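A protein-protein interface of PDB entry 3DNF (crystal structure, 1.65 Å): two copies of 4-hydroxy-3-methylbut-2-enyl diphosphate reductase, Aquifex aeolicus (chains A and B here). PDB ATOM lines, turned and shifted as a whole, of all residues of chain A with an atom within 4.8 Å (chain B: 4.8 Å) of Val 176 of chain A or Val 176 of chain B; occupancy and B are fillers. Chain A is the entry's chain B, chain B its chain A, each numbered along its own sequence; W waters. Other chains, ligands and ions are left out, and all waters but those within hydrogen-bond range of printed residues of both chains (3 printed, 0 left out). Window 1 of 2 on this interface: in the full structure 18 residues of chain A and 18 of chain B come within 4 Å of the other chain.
Among the printed residues, merely in contact across the chains: Lys 173 of chain A with Gly 177 of chain B (3.6 Å), Val 176 of chain A with Val 176 of chain B (3.8 Å) and Gly 177 of chain A with Lys 173 of chain B (3.5 Å).
Printed residues of chain A within 4 Å of Glu 178 of chain B: Lys 173 (2.8 Å). Printed residues of chain B within 4 Å of Gly 177 of chain A: Lys 173 (3.5 Å). Ile 161 of chain A touches none of the printed residues of chain B. Ile 179 of chain B touches none of the printed residues of chain A. The nearest printed residue of chain A that does not touch Val 176 of chain B is Ala 180 of chain A (4.004 Å).
Of the 11 printed residues of chain A, 5 touch a printed residue of chain B. Among the printed residues, Asp or Glu carboxylates within 4 Å of a Lys or Arg side-chain nitrogen of the other chain: Lys 173 of chain A with Glu 174 of chain B, Lys 173 of chain A with Glu 178 of chain B, Glu 174 of chain A with Lys 173 of chain B and Glu 178 of chain A with Lys 173 of chain B.
OE1 of Glu 178 of chain A is in salt-bridge range of NZ of Lys 173 of chain B. The side-chain carboxylate (OE1) of Glu 178 of chain B is in salt-bridge range of the side-chain amino group (NZ) of Lys 173 of chain A, 2.8 Å away. NZ of Lys 173 of chain B is in salt-bridge range of OE2 of Glu 174 of chain A (2.8 Å). NZ of Lys 173 of chain A is in salt-bridge range of OE2 of Glu 174 of chain B, 2.7 Å away.
Water W3 lies within hydrogen-bond range of OE2 of Glu 174 of chain A (2.4 Å), NZ of Lys 173 of chain B (2.8 Å) and OE1 of Glu 178 of chain A (3.0 Å). Water W2 bridges O of Lys 173 of chain A and O of Lys 173 of chain B. Water W1 bridges OE1 of Glu 174 of chain B (3.4 Å) and NZ of Lys 173 of chain A (3.5 Å).
Lys 173 of chain A touches Glu 174 of chain B, and with the chains exchanged Glu 174 of chain A touches Lys 173 of chain B. Lys 173 of chain A touches Gly 177 of chain B, and with the chains exchanged Gly 177 of chain A touches Lys 173 of chain B. Lys 173 of chain A touches Glu 178 of chain B, and with the chains exchanged Glu 178 of chain A touches Lys 173 of chain B. Val 176 of chain B touches its own counterpart, Val 176 of chain A. 11 positions are printed for both chains.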
ATOM      1  N   ILE A 161      24.516  10.570  10.030  1.00  0.00           N
ATOM      2  CA  ILE A 161      23.793  10.038   8.917  1.00  0.00           C
ATOM      3  C   ILE A 161      22.419  10.669   8.804  1.00  0.00           C
ATOM      4  O   ILE A 161      21.671  10.685   9.796  1.00  0.00           O
ATOM      5  CB  ILE A 161      23.689   8.484   8.996  1.00  0.00           C
ATOM      6  CG1 ILE A 161      25.091   7.913   9.128  1.00  0.00           C
ATOM      7  CG2 ILE A 161      22.963   7.870   7.774  1.00  0.00           C
ATOM      8  CD1 ILE A 161      25.131   6.420   9.425  1.00  0.00           C
ATOM      9  N   PHE A 172      18.207   2.481   4.002  1.00  0.00           N
ATOM     10  CA  PHE A 172      18.664   3.370   5.069  1.00  0.00           C
ATOM     11  C   PHE A 172      19.027   2.548   6.305  1.00  0.00           C
ATOM     12  O   PHE A 172      20.065   2.752   6.901  1.00  0.00           O
ATOM     13  CB  PHE A 172      17.553   4.313   5.411  1.00  0.00           C
ATOM     14  CG  PHE A 172      17.963   5.375   6.380  1.00  0.00           C
ATOM     15  CD1 PHE A 172      18.895   6.356   5.994  1.00  0.00           C
ATOM     16  CD2 PHE A 172      17.474   5.356   7.696  1.00  0.00           C
ATOM     17  CE1 PHE A 172      19.285   7.325   6.876  1.00  0.00           C
ATOM     18  CE2 PHE A 172      17.852   6.354   8.595  1.00  0.00           C
ATOM     19  CZ  PHE A 172      18.779   7.327   8.182  1.00  0.00           C
ATOM     20  N   LYS A 173      18.182   1.563   6.636  1.00  0.00           N
ATOM     21  CA  LYS A 173      18.404   0.674   7.788  1.00  0.00           C
ATOM     22  C   LYS A 173      19.736  -0.106   7.644  1.00  0.00           C
ATOM     23  O   LYS A 173      20.505  -0.230   8.606  1.00  0.00           O
ATOM     24  CB  LYS A 173      17.197  -0.256   7.991  1.00  0.00           C
ATOM     25  CG  LYS A 173      17.441  -1.366   8.973  1.00  0.00           C
ATOM     26  CD  LYS A 173      16.207  -2.197   9.191  1.00  0.00           C
ATOM     27  CE  LYS A 173      16.529  -3.318  10.147  1.00  0.00           C
ATOM     28  NZ  LYS A 173      15.346  -4.204  10.272  1.00  0.00           N
ATOM     29  N   GLU A 174      19.996  -0.591   6.425  1.00  0.00           N
ATOM     30  CA  GLU A 174      21.218  -1.320   6.098  1.00  0.00           C
ATOM     31  C   GLU A 174      22.473  -0.462   6.235  1.00  0.00           C
ATOM     32  O   GLU A 174      23.470  -0.937   6.815  1.00  0.00           O
ATOM     33  CB  GLU A 174      21.120  -1.916   4.673  1.00  0.00           C
ATOM     34  CG  GLU A 174      22.381  -2.608   4.167  1.00  0.00           C
ATOM     35  CD  GLU A 174      22.661  -3.919   4.868  1.00  0.00           C
ATOM     36  OE1 GLU A 174      21.751  -4.450   5.549  1.00  0.00           O
ATOM     37  OE2 GLU A 174      23.804  -4.427   4.758  1.00  0.00           O
ATOM     38  N   VAL A 175      22.434   0.752   5.658  1.00  0.00           N
ATOM     39  CA  VAL A 175      23.559   1.700   5.706  1.00  0.00           C
ATOM     40  C   VAL A 175      23.886   2.084   7.153  1.00  0.00           C
ATOM     41  O   VAL A 175      25.051   2.096   7.563  1.00  0.00           O
ATOM     42  CB  VAL A 175      23.276   3.020   4.900  1.00  0.00           C
ATOM     43  CG1 VAL A 175      24.425   4.045   5.159  1.00  0.00           C
ATOM     44  CG2 VAL A 175      23.167   2.714   3.446  1.00  0.00           C
ATOM     45  N   VAL A 176      22.854   2.439   7.907  1.00  0.00           N
ATOM     46  CA  VAL A 176      23.048   2.813   9.310  1.00  0.00           C
ATOM     47  C   VAL A 176      23.704   1.669  10.112  1.00  0.00           C
ATOM     48  O   VAL A 176      24.681   1.874  10.821  1.00  0.00           O
ATOM     49  CB  VAL A 176      21.713   3.264   9.965  1.00  0.00           C
ATOM     50  CG1 VAL A 176      21.845   3.321  11.510  1.00  0.00           C
ATOM     51  CG2 VAL A 176      21.225   4.614   9.363  1.00  0.00           C
ATOM     52  N   GLY A 177      23.179   0.458   9.978  1.00  0.00           N
ATOM     53  CA  GLY A 177      23.670  -0.689  10.720  1.00  0.00           C
ATOM     54  C   GLY A 177      25.101  -1.002  10.322  1.00  0.00           C
ATOM     55  O   GLY A 177      25.949  -1.237  11.170  1.00  0.00           O
ATOM     56  N   GLU A 178      25.369  -0.950   9.017  1.00  0.00           N
ATOM     57  CA  GLU A 178      26.693  -1.270   8.521  1.00  0.00           C
ATOM     58  C   GLU A 178      27.740  -0.268   8.992  1.00  0.00           C
ATOM     59  O   GLU A 178      28.769  -0.653   9.561  1.00  0.00           O
ATOM     60  CB  GLU A 178      26.680  -1.403   6.990  1.00  0.00           C
ATOM     61  CG  GLU A 178      27.991  -1.984   6.420  1.00  0.00           C
ATOM     62  CD  GLU A 178      28.339  -3.403   6.901  1.00  0.00           C
ATOM     63  OE1 GLU A 178      27.436  -4.210   7.221  1.00  0.00           O
ATOM     64  OE2 GLU A 178      29.548  -3.710   6.952  1.00  0.00           O
ATOM     65  N   ILE A 179      27.484   1.024   8.791  1.00  0.00           N
ATOM     66  CA  ILE A 179      28.439   2.047   9.256  1.00  0.00           C
ATOM     67  C   ILE A 179      28.718   1.918  10.771  1.00  0.00           C
ATOM     68  O   ILE A 179      29.870   2.000  11.193  1.00  0.00           O
ATOM     69  CB  ILE A 179      28.007   3.475   8.840  1.00  0.00           C
ATOM     70  CG1 ILE A 179      28.093   3.619   7.308  1.00  0.00           C
ATOM     71  CG2 ILE A 179      28.858   4.586   9.502  1.00  0.00           C
ATOM     72  CD1 ILE A 179      27.528   4.917   6.793  1.00  0.00           C
ATOM     73  N   ALA A 180      27.674   1.669  11.560  1.00  0.00           N
ATOM     74  CA  ALA A 180      27.798   1.505  13.018  1.00  0.00           C
ATOM     75  C   ALA A 180      28.773   0.384  13.438  1.00  0.00           C
ATOM     76  O   ALA A 180      29.391   0.432  14.512  1.00  0.00           O
ATOM     77  CB  ALA A 180      26.447   1.263  13.620  1.00  0.00           C
ATOM     78  N   VAL A 188      22.482   9.345  13.988  1.00  0.00           N
ATOM     79  CA  VAL A 188      21.529   9.319  12.910  1.00  0.00           C
ATOM     80  C   VAL A 188      20.410  10.273  13.203  1.00  0.00           C
ATOM     81  O   VAL A 188      19.829  10.259  14.292  1.00  0.00           O
ATOM     82  CB  VAL A 188      20.888   7.903  12.773  1.00  0.00           C
ATOM     83  CG1 VAL A 188      19.868   7.823  11.609  1.00  0.00           C
ATOM     84  CG2 VAL A 188      21.975   6.834  12.681  1.00  0.00           C
ATOM     85  N   ILE B 161      22.698   4.083  21.916  1.00  0.00           N
ATOM     86  CA  ILE B 161      22.849   2.618  21.834  1.00  0.00           C
ATOM     87  C   ILE B 161      24.294   2.164  22.084  1.00  0.00           C
ATOM     88  O   ILE B 161      25.227   2.629  21.434  1.00  0.00           O
ATOM     89  CB  ILE B 161      22.368   2.073  20.511  1.00  0.00           C
ATOM     90  CG1 ILE B 161      20.924   2.547  20.154  1.00  0.00           C
ATOM     91  CG2 ILE B 161      22.421   0.521  20.540  1.00  0.00           C
ATOM     92  CD1 ILE B 161      20.466   2.124  18.760  1.00  0.00           C
ATOM     93  N   PHE B 172      23.465  -6.748  16.587  1.00  0.00           N
ATOM     94  CA  PHE B 172      23.718  -5.343  16.925  1.00  0.00           C
ATOM     95  C   PHE B 172      23.335  -4.432  15.729  1.00  0.00           C
ATOM     96  O   PHE B 172      22.613  -3.445  15.912  1.00  0.00           O
ATOM     97  CB  PHE B 172      25.179  -5.128  17.320  1.00  0.00           C
ATOM     98  CG  PHE B 172      25.470  -3.730  17.811  1.00  0.00           C
ATOM     99  CD1 PHE B 172      24.934  -3.263  19.013  1.00  0.00           C
ATOM    100  CD2 PHE B 172      26.278  -2.889  17.037  1.00  0.00           C
ATOM    101  CE1 PHE B 172      25.230  -1.950  19.487  1.00  0.00           C
ATOM    102  CE2 PHE B 172      26.544  -1.561  17.473  1.00  0.00           C
ATOM    103  CZ  PHE B 172      26.031  -1.108  18.703  1.00  0.00           C
ATOM    104  N   LYS B 173      23.787  -4.797  14.531  1.00  0.00           N
ATOM    105  CA  LYS B 173      23.470  -4.069  13.299  1.00  0.00           C
ATOM    106  C   LYS B 173      21.942  -3.997  13.128  1.00  0.00           C
ATOM    107  O   LYS B 173      21.382  -2.969  12.714  1.00  0.00           O
ATOM    108  CB  LYS B 173      24.116  -4.791  12.096  1.00  0.00           C
ATOM    109  CG  LYS B 173      23.774  -4.237  10.728  1.00  0.00           C
ATOM    110  CD  LYS B 173      24.468  -5.044   9.657  1.00  0.00           C
ATOM    111  CE  LYS B 173      24.128  -4.558   8.269  1.00  0.00           C
ATOM    112  NZ  LYS B 173      24.912  -5.271   7.223  1.00  0.00           N
ATOM    113  N   GLU B 174      21.267  -5.108  13.412  1.00  0.00           N
ATOM    114  CA  GLU B 174      19.814  -5.174  13.241  1.00  0.00           C
ATOM    115  C   GLU B 174      19.069  -4.219  14.202  1.00  0.00           C
ATOM    116  O   GLU B 174      18.151  -3.484  13.784  1.00  0.00           O
ATOM    117  CB  GLU B 174      19.316  -6.606  13.449  1.00  0.00           C
ATOM    118  CG  GLU B 174      17.798  -6.734  13.413  1.00  0.00           C
ATOM    119  CD  GLU B 174      17.177  -6.480  12.047  1.00  0.00           C
ATOM    120  OE1 GLU B 174      17.889  -6.555  11.012  1.00  0.00           O
ATOM    121  OE2 GLU B 174      15.946  -6.231  11.993  1.00  0.00           O
ATOM    122  N   VAL B 175      19.438  -4.268  15.477  1.00  0.00           N
ATOM    123  CA  VAL B 175      18.859  -3.374  16.500  1.00  0.00           C
ATOM    124  C   VAL B 175      19.080  -1.889  16.163  1.00  0.00           C
ATOM    125  O   VAL B 175      18.161  -1.062  16.178  1.00  0.00           O
ATOM    126  CB  VAL B 175      19.395  -3.699  17.911  1.00  0.00           C
ATOM    127  CG1 VAL B 175      18.998  -2.611  18.940  1.00  0.00           C
ATOM    128  CG2 VAL B 175      18.912  -5.055  18.353  1.00  0.00           C
ATOM    129  N   VAL B 176      20.317  -1.559  15.846  1.00  0.00           N
ATOM    130  CA  VAL B 176      20.659  -0.203  15.512  1.00  0.00           C
ATOM    131  C   VAL B 176      19.843   0.296  14.303  1.00  0.00           C
ATOM    132  O   VAL B 176      19.309   1.412  14.350  1.00  0.00           O
ATOM    133  CB  VAL B 176      22.199  -0.099  15.245  1.00  0.00           C
ATOM    134  CG1 VAL B 176      22.550   1.192  14.537  1.00  0.00           C
ATOM    135  CG2 VAL B 176      22.981  -0.322  16.513  1.00  0.00           C
ATOM    136  N   GLY B 177      19.742  -0.505  13.239  1.00  0.00           N
ATOM    137  CA  GLY B 177      19.057  -0.052  12.033  1.00  0.00           C
ATOM    138  C   GLY B 177      17.567   0.032  12.321  1.00  0.00           C
ATOM    139  O   GLY B 177      16.918   0.941  11.849  1.00  0.00           O
ATOM    140  N   GLU B 178      17.032  -0.911  13.120  1.00  0.00           N
ATOM    141  CA  GLU B 178      15.588  -0.932  13.368  1.00  0.00           C
ATOM    142  C   GLU B 178      15.170   0.273  14.217  1.00  0.00           C
ATOM    143  O   GLU B 178      14.200   0.967  13.882  1.00  0.00           O
ATOM    144  CB  GLU B 178      15.123  -2.245  14.006  1.00  0.00           C
ATOM    145  CG  GLU B 178      13.594  -2.366  14.091  1.00  0.00           C
ATOM    146  CD  GLU B 178      12.877  -2.431  12.740  1.00  0.00           C
ATOM    147  OE1 GLU B 178      13.498  -2.640  11.672  1.00  0.00           O
ATOM    148  OE2 GLU B 178      11.634  -2.291  12.734  1.00  0.00           O
ATOM    149  N   ILE B 179      15.896   0.515  15.293  1.00  0.00           N
ATOM    150  CA  ILE B 179      15.592   1.645  16.178  1.00  0.00           C
ATOM    151  C   ILE B 179      15.666   2.981  15.362  1.00  0.00           C
ATOM    152  O   ILE B 179      14.772   3.823  15.484  1.00  0.00           O
ATOM    153  CB  ILE B 179      16.452   1.640  17.427  1.00  0.00           C
ATOM    154  CG1 ILE B 179      16.079   0.460  18.341  1.00  0.00           C
ATOM    155  CG2 ILE B 179      16.378   3.010  18.173  1.00  0.00           C
ATOM    156  CD1 ILE B 179      16.932   0.390  19.611  1.00  0.00           C
ATOM    157  N   ALA B 180      16.695   3.128  14.536  1.00  0.00           N
ATOM    158  CA  ALA B 180      16.841   4.288  13.644  1.00  0.00           C
ATOM    159  C   ALA B 180      15.616   4.577  12.770  1.00  0.00           C
ATOM    160  O   ALA B 180      15.322   5.743  12.467  1.00  0.00           O
ATOM    161  CB  ALA B 180      18.101   4.153  12.790  1.00  0.00           C
ATOM    162  N   VAL B 188      24.922   5.940  18.330  1.00  0.00           N
ATOM    163  CA  VAL B 188      25.510   4.642  18.608  1.00  0.00           C
ATOM    164  C   VAL B 188      26.973   4.855  19.002  1.00  0.00           C
ATOM    165  O   VAL B 188      27.747   5.554  18.326  1.00  0.00           O
ATOM    166  CB  VAL B 188      25.424   3.740  17.354  1.00  0.00           C
ATOM    167  CG1 VAL B 188      26.010   2.331  17.635  1.00  0.00           C
ATOM    168  CG2 VAL B 188      23.974   3.648  16.796  1.00  0.00           C
HETATM  169  O   HOH W   1      15.882  -7.031   8.362  1.00  0.00           O
HETATM  170  O   HOH W   2      20.662  -2.665  10.005  1.00  0.00           O
HETATM  171  O   HOH W   3      26.139  -5.137   4.702  1.00  0.00           O
